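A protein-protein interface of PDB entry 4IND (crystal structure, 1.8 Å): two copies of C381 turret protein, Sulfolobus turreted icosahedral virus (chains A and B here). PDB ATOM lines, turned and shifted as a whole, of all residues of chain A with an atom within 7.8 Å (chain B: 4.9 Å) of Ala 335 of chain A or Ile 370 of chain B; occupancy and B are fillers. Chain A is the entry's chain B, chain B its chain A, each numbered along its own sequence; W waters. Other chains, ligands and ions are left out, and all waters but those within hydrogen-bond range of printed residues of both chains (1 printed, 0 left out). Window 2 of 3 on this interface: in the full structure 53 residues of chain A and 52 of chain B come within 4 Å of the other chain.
The backbone carbonyl oxygen (O) of Tyr 301 of chain B is in hydrogen-bond range of the backbone NH (N) of Val 372 of chain B.
O of Ser 303 of chain B lies within hydrogen-bond range of N of Ile 370 of chain B, at 2.8 Å.
The side-chain carboxylate of Asp 332 of chain A sits at hydrogen-bond distance from the side-chain amide nitrogen of Gln 315 of chain A (3.3 Å).
The indole nitrogen (NE1) of Trp 331 of chain A is in hydrogen-bond range of the backbone carbonyl oxygen (O) of Gly 337 of chain A, at 3.0 Å.
The side-chain carboxylate of Asp 332 of chain A lies within hydrogen-bond range of the backbone NH of Ile 334 of chain A.
The backbone NH (N) of Ala 335 of chain A sits at hydrogen-bond distance from the side-chain carboxylate (OD1) of Asp 332 of chain A (3.0 Å).
Among the printed residues, pairs that only touch across the chains: Trp 331 of chain A with Phe 271 of chain B (3.4 Å), Asp 332 of chain A with Phe 271 of chain B (3.4 Å), Gly 336 of chain A with Ile 370 of chain B (3.8 Å), Ala 335 of chain A with Ile 370 of chain B (3.8 Å), Trp 331 of chain A with Tyr 301 of chain B (3.9 Å), Trp 331 of chain A with Val 372 of chain B (3.9 Å) and Gly 336 of chain A with Phe 271 of chain B (3.96 Å).
Leu 307 of chain A touches none of the printed residues of chain B.
Of the printed residues of chain B, Trp 331 of chain A touches Phe 271 (3.4 Å), Tyr 301 (3.9 Å) and Val 372 (3.9 Å).
Of the printed residues of chain B, Asp 332 of chain A touches Phe 271.
Ala 335 of chain A touches just one residue of chain B: Ile 370 (3.8 Å).
Gly 337 of chain A touches none of the printed residues of chain B.
Of the printed residues of chain A, Phe 271 of chain B touches Trp 331, Asp 332 and Gly 336.
Of chain A, only Ala 335 and Gly 336 come within 4 Å of Ile 370 of chain B.
Of the printed residues of chain A, Val 372 of chain B touches Trp 331.
The nearest residue of chain B that does not touch Ala 335 of chain A is Phe 271 of chain B (4.2 Å).
The nearest residue of chain A that does not touch Ile 370 of chain B is Trp 331 of chain A (5.2 Å).
Hydrophobic or aromatic side chains of chain B that line the printed part of chain A: Phe 271, Tyr 301, Ile 370 and Val 372.
Of the 12 printed residues of chain A, 4 touch a printed residue of chain B.
Among the printed residues, no Asp or Glu carboxylate lies within 4 Å of a Lys or Arg side-chain nitrogen of the other chain.
No position is printed for both chains.
Water W1 lies within hydrogen-bond range of the side-chain hydroxyl of Tyr 301 of chain B (2.5 Å) and the backbone carbonyl oxygen of Gly 336 of chain A (3.0 Å).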
ATOM      1  N   LEU A 307       8.754  18.018   4.108  1.00  0.00           N
ATOM      2  CA  LEU A 307       7.903  18.410   2.987  1.00  0.00           C
ATOM      3  C   LEU A 307       8.584  19.428   2.080  1.00  0.00           C
ATOM      4  O   LEU A 307       9.151  20.416   2.545  1.00  0.00           O
ATOM      5  CB  LEU A 307       6.571  18.973   3.483  1.00  0.00           C
ATOM      6  CG  LEU A 307       5.605  17.958   4.079  1.00  0.00           C
ATOM      7  CD1 LEU A 307       4.301  18.632   4.489  1.00  0.00           C
ATOM      8  CD2 LEU A 307       5.324  16.826   3.096  1.00  0.00           C
ATOM      9  N   THR A 312       3.706  15.717  -3.519  1.00  0.00           N
ATOM     10  CA  THR A 312       2.432  16.084  -4.132  1.00  0.00           C
ATOM     11  C   THR A 312       1.246  15.582  -3.323  1.00  0.00           C
ATOM     12  O   THR A 312       0.130  16.082  -3.458  1.00  0.00           O
ATOM     13  CB  THR A 312       2.314  15.502  -5.552  1.00  0.00           C
ATOM     14  OG1 THR A 312       2.416  14.075  -5.483  1.00  0.00           O
ATOM     15  CG2 THR A 312       3.409  16.051  -6.454  1.00  0.00           C
ATOM     16  N   CYS A 314       0.310  13.967   0.762  1.00  0.00           N
ATOM     17  CA  CYS A 314       0.711  13.547   2.091  1.00  0.00           C
ATOM     18  C   CYS A 314      -0.513  13.658   2.975  1.00  0.00           C
ATOM     19  O   CYS A 314      -0.792  14.723   3.523  1.00  0.00           O
ATOM     20  CB  CYS A 314       1.868  14.422   2.610  1.00  0.00           C
ATOM     21  SG  CYS A 314       2.565  13.843   4.189  1.00  0.00           S
ATOM     22  N   GLN A 315      -1.265  12.561   3.065  1.00  0.00           N
ATOM     23  CA  GLN A 315      -2.501  12.526   3.830  1.00  0.00           C
ATOM     24  C   GLN A 315      -2.444  11.448   4.891  1.00  0.00           C
ATOM     25  O   GLN A 315      -2.105  10.299   4.601  1.00  0.00           O
ATOM     26  CB  GLN A 315      -3.698  12.266   2.912  1.00  0.00           C
ATOM     27  CG  GLN A 315      -3.918  13.347   1.864  1.00  0.00           C
ATOM     28  CD  GLN A 315      -4.983  12.975   0.858  1.00  0.00           C
ATOM     29  OE1 GLN A 315      -5.153  11.804   0.525  1.00  0.00           O
ATOM     30  NE2 GLN A 315      -5.712  13.975   0.369  1.00  0.00           N
ATOM     31  N   TRP A 331      -6.187  14.287   8.132  1.00  0.00           N
ATOM     32  CA  TRP A 331      -5.384  15.493   7.951  1.00  0.00           C
ATOM     33  C   TRP A 331      -4.609  15.432   6.658  1.00  0.00           C
ATOM     34  O   TRP A 331      -4.056  14.387   6.308  1.00  0.00           O
ATOM     35  CB  TRP A 331      -4.435  15.742   9.125  1.00  0.00           C
ATOM     36  CG  TRP A 331      -3.809  17.126   9.036  1.00  0.00           C
ATOM     37  CD1 TRP A 331      -2.536  17.442   8.626  1.00  0.00           C
ATOM     38  CD2 TRP A 331      -4.451  18.368   9.323  1.00  0.00           C
ATOM     39  NE1 TRP A 331      -2.355  18.800   8.654  1.00  0.00           N
ATOM     40  CE2 TRP A 331      -3.524  19.397   9.077  1.00  0.00           C
ATOM     41  CE3 TRP A 331      -5.737  18.717   9.767  1.00  0.00           C
ATOM     42  CZ2 TRP A 331      -3.824  20.750   9.259  1.00  0.00           C
ATOM     43  CZ3 TRP A 331      -6.042  20.062   9.949  1.00  0.00           C
ATOM     44  CH2 TRP A 331      -5.089  21.059   9.705  1.00  0.00           C
ATOM     45  N   ASP A 332      -4.599  16.547   5.934  1.00  0.00           N
ATOM     46  CA  ASP A 332      -3.841  16.663   4.694  1.00  0.00           C
ATOM     47  C   ASP A 332      -2.715  17.657   4.934  1.00  0.00           C
ATOM     48  O   ASP A 332      -2.963  18.844   5.112  1.00  0.00           O
ATOM     49  CB  ASP A 332      -4.763  17.141   3.575  1.00  0.00           C
ATOM     50  CG  ASP A 332      -4.078  17.190   2.239  1.00  0.00           C
ATOM     51  OD1 ASP A 332      -2.852  17.423   2.209  1.00  0.00           O
ATOM     52  OD2 ASP A 332      -4.763  17.013   1.215  1.00  0.00           O
ATOM     53  N   PHE A 333      -1.479  17.168   4.977  1.00  0.00           N
ATOM     54  CA  PHE A 333      -0.347  18.012   5.337  1.00  0.00           C
ATOM     55  C   PHE A 333       0.009  19.008   4.248  1.00  0.00           C
ATOM     56  O   PHE A 333       0.637  20.028   4.527  1.00  0.00           O
ATOM     57  CB  PHE A 333       0.865  17.157   5.733  1.00  0.00           C
ATOM     58  CG  PHE A 333       0.629  16.344   6.973  1.00  0.00           C
ATOM     59  CD1 PHE A 333       0.836  16.902   8.229  1.00  0.00           C
ATOM     60  CD2 PHE A 333       0.165  15.042   6.892  1.00  0.00           C
ATOM     61  CE1 PHE A 333       0.608  16.164   9.394  1.00  0.00           C
ATOM     62  CE2 PHE A 333      -0.080  14.290   8.049  1.00  0.00           C
ATOM     63  CZ  PHE A 333       0.144  14.854   9.301  1.00  0.00           C
ATOM     64  N   ILE A 334      -0.384  18.717   3.009  1.00  0.00           N
ATOM     65  CA  ILE A 334      -0.172  19.669   1.923  1.00  0.00           C
ATOM     66  C   ILE A 334      -1.210  20.788   2.007  1.00  0.00           C
ATOM     67  O   ILE A 334      -0.865  21.958   2.074  1.00  0.00           O
ATOM     68  CB  ILE A 334      -0.272  18.999   0.544  1.00  0.00           C
ATOM     69  CG1 ILE A 334       0.679  17.802   0.441  1.00  0.00           C
ATOM     70  CG2 ILE A 334      -0.003  20.001  -0.552  1.00  0.00           C
ATOM     71  CD1 ILE A 334       2.127  18.134   0.691  1.00  0.00           C
ATOM     72  N   ALA A 335      -2.486  20.411   2.018  1.00  0.00           N
ATOM     73  CA  ALA A 335      -3.579  21.377   1.986  1.00  0.00           C
ATOM     74  C   ALA A 335      -3.731  22.117   3.300  1.00  0.00           C
ATOM     75  O   ALA A 335      -4.104  23.290   3.313  1.00  0.00           O
ATOM     76  CB  ALA A 335      -4.881  20.677   1.627  1.00  0.00           C
ATOM     77  N   GLY A 336      -3.448  21.431   4.406  1.00  0.00           N
ATOM     78  CA  GLY A 336      -3.693  21.981   5.729  1.00  0.00           C
ATOM     79  C   GLY A 336      -2.475  22.513   6.467  1.00  0.00           C
ATOM     80  O   GLY A 336      -2.619  23.259   7.435  1.00  0.00           O
ATOM     81  N   GLY A 337      -1.275  22.141   6.023  1.00  0.00           N
ATOM     82  CA  GLY A 337      -0.065  22.558   6.717  1.00  0.00           C
ATOM     83  C   GLY A 337       0.628  21.414   7.437  1.00  0.00           C
ATOM     84  O   GLY A 337       0.042  20.363   7.665  1.00  0.00           O
ATOM     85  N   SER A 338       1.883  21.632   7.810  1.00  0.00           N
ATOM     86  CA  SER A 338       2.759  20.554   8.274  1.00  0.00           C
ATOM     87  C   SER A 338       2.425  19.994   9.664  1.00  0.00           C
ATOM     88  O   SER A 338       2.995  18.987  10.081  1.00  0.00           O
ATOM     89  CB  SER A 338       4.205  21.027   8.257  1.00  0.00           C
ATOM     90  OG  SER A 338       4.346  22.167   9.083  1.00  0.00           O
ATOM     91  N   PHE B 271     -11.244  15.281   7.199  1.00  0.00           N
ATOM     92  CA  PHE B 271     -10.663  16.500   6.697  1.00  0.00           C
ATOM     93  C   PHE B 271     -11.172  16.604   5.265  1.00  0.00           C
ATOM     94  O   PHE B 271     -10.940  15.709   4.449  1.00  0.00           O
ATOM     95  CB  PHE B 271      -9.141  16.363   6.708  1.00  0.00           C
ATOM     96  CG  PHE B 271      -8.402  17.544   6.151  1.00  0.00           C
ATOM     97  CD1 PHE B 271      -7.720  18.409   7.002  1.00  0.00           C
ATOM     98  CD2 PHE B 271      -8.349  17.778   4.781  1.00  0.00           C
ATOM     99  CE1 PHE B 271      -7.003  19.502   6.501  1.00  0.00           C
ATOM    100  CE2 PHE B 271      -7.632  18.873   4.260  1.00  0.00           C
ATOM    101  CZ  PHE B 271      -6.957  19.732   5.124  1.00  0.00           C
ATOM    102  N   VAL B 272     -11.868  17.692   4.955  1.00  0.00           N
ATOM    103  CA  VAL B 272     -12.459  17.841   3.631  1.00  0.00           C
ATOM    104  C   VAL B 272     -12.110  19.193   3.048  1.00  0.00           C
ATOM    105  O   VAL B 272     -11.826  20.153   3.769  1.00  0.00           O
ATOM    106  CB  VAL B 272     -13.994  17.609   3.647  1.00  0.00           C
ATOM    107  CG1 VAL B 272     -14.699  18.710   4.410  1.00  0.00           C
ATOM    108  CG2 VAL B 272     -14.525  17.533   2.226  1.00  0.00           C
ATOM    109  N   THR B 273     -12.108  19.259   1.727  1.00  0.00           N
ATOM    110  CA  THR B 273     -11.708  20.471   1.036  1.00  0.00           C
ATOM    111  C   THR B 273     -12.755  20.810  -0.017  1.00  0.00           C
ATOM    112  O   THR B 273     -13.365  19.917  -0.611  1.00  0.00           O
ATOM    113  CB  THR B 273     -10.324  20.304   0.380  1.00  0.00           C
ATOM    114  OG1 THR B 273      -9.818  21.589   0.018  1.00  0.00           O
ATOM    115  CG2 THR B 273     -10.421  19.437  -0.857  1.00  0.00           C
ATOM    116  N   TYR B 301     -12.443  22.574  13.079  1.00  0.00           N
ATOM    117  CA  TYR B 301     -11.444  23.471  12.493  1.00  0.00           C
ATOM    118  C   TYR B 301     -11.814  23.833  11.065  1.00  0.00           C
ATOM    119  O   TYR B 301     -12.305  22.991  10.310  1.00  0.00           O
ATOM    120  CB  TYR B 301     -10.086  22.788  12.491  1.00  0.00           C
ATOM    121  CG  TYR B 301      -8.973  23.608  11.846  1.00  0.00           C
ATOM    122  CD1 TYR B 301      -8.348  24.631  12.547  1.00  0.00           C
ATOM    123  CD2 TYR B 301      -8.535  23.332  10.555  1.00  0.00           C
ATOM    124  CE1 TYR B 301      -7.314  25.382  11.961  1.00  0.00           C
ATOM    125  CE2 TYR B 301      -7.514  24.067   9.955  1.00  0.00           C
ATOM    126  CZ  TYR B 301      -6.912  25.096  10.665  1.00  0.00           C
ATOM    127  OH  TYR B 301      -5.888  25.829  10.085  1.00  0.00           O
ATOM    128  N   ALA B 302     -11.582  25.087  10.698  1.00  0.00           N
ATOM    129  CA  ALA B 302     -11.803  25.529   9.327  1.00  0.00           C
ATOM    130  C   ALA B 302     -10.776  26.567   8.911  1.00  0.00           C
ATOM    131  O   ALA B 302     -10.319  27.375   9.725  1.00  0.00           O
ATOM    132  CB  ALA B 302     -13.216  26.072   9.140  1.00  0.00           C
ATOM    133  N   SER B 303     -10.416  26.543   7.636  1.00  0.00           N
ATOM    134  CA  SER B 303      -9.435  27.475   7.110  1.00  0.00           C
ATOM    135  C   SER B 303      -9.754  27.758   5.652  1.00  0.00           C
ATOM    136  O   SER B 303     -10.287  26.899   4.945  1.00  0.00           O
ATOM    137  CB  SER B 303      -8.039  26.875   7.227  1.00  0.00           C
ATOM    138  OG  SER B 303      -7.059  27.825   6.891  1.00  0.00           O
ATOM    139  N   THR B 368     -10.289  28.244  -1.381  1.00  0.00           N
ATOM    140  CA  THR B 368     -10.427  26.853  -0.999  1.00  0.00           C
ATOM    141  C   THR B 368     -10.650  26.752   0.490  1.00  0.00           C
ATOM    142  O   THR B 368      -9.838  27.246   1.277  1.00  0.00           O
ATOM    143  CB  THR B 368      -9.193  26.044  -1.402  1.00  0.00           C
ATOM    144  OG1 THR B 368      -9.059  26.073  -2.830  1.00  0.00           O
ATOM    145  CG2 THR B 368      -9.326  24.593  -0.938  1.00  0.00           C
ATOM    146  N   LEU B 369     -11.768  26.124   0.862  1.00  0.00           N
ATOM    147  CA  LEU B 369     -12.116  25.895   2.239  1.00  0.00           C
ATOM    148  C   LEU B 369     -11.612  24.513   2.630  1.00  0.00           C
ATOM    149  O   LEU B 369     -11.782  23.553   1.890  1.00  0.00           O
ATOM    150  CB  LEU B 369     -13.639  25.941   2.404  1.00  0.00           C
ATOM    151  CG  LEU B 369     -14.200  25.492   3.750  1.00  0.00           C
ATOM    152  CD1 LEU B 369     -13.806  26.480   4.819  1.00  0.00           C
ATOM    153  CD2 LEU B 369     -15.730  25.327   3.694  1.00  0.00           C
ATOM    154  N   ILE B 370     -10.964  24.418   3.783  1.00  0.00           N
ATOM    155  CA  ILE B 370     -10.716  23.119   4.377  1.00  0.00           C
ATOM    156  C   ILE B 370     -11.456  23.077   5.704  1.00  0.00           C
ATOM    157  O   ILE B 370     -11.617  24.100   6.386  1.00  0.00           O
ATOM    158  CB  ILE B 370      -9.222  22.807   4.562  1.00  0.00           C
ATOM    159  CG1 ILE B 370      -8.616  23.689   5.642  1.00  0.00           C
ATOM    160  CG2 ILE B 370      -8.455  22.981   3.264  1.00  0.00           C
ATOM    161  CD1 ILE B 370      -7.107  23.614   5.670  1.00  0.00           C
ATOM    162  N   LEU B 371     -11.921  21.889   6.053  1.00  0.00           N
ATOM    163  CA  LEU B 371     -12.778  21.716   7.207  1.00  0.00           C
ATOM    164  C   LEU B 371     -12.473  20.358   7.826  1.00  0.00           C
ATOM    165  O   LEU B 371     -12.288  19.368   7.108  1.00  0.00           O
ATOM    166  CB  LEU B 371     -14.237  21.821   6.763  1.00  0.00           C
ATOM    167  CG  LEU B 371     -15.332  21.532   7.783  1.00  0.00           C
ATOM    168  CD1 LEU B 371     -15.274  22.550   8.910  1.00  0.00           C
ATOM    169  CD2 LEU B 371     -16.697  21.545   7.107  1.00  0.00           C
ATOM    170  N   VAL B 372     -12.353  20.328   9.152  1.00  0.00           N
ATOM    171  CA  VAL B 372     -12.294  19.071   9.877  1.00  0.00           C
ATOM    172  C   VAL B 372     -13.568  18.979  10.684  1.00  0.00           C
ATOM    173  O   VAL B 372     -13.900  19.905  11.426  1.00  0.00           O
ATOM    174  CB  VAL B 372     -11.090  19.012  10.825  1.00  0.00           C
ATOM    175  CG1 VAL B 372     -11.159  17.744  11.654  1.00  0.00           C
ATOM    176  CG2 VAL B 372      -9.793  19.062  10.022  1.00  0.00           C
HETATM  177  O   HOH W   1      -5.095  24.945   7.867  1.00  0.00           O
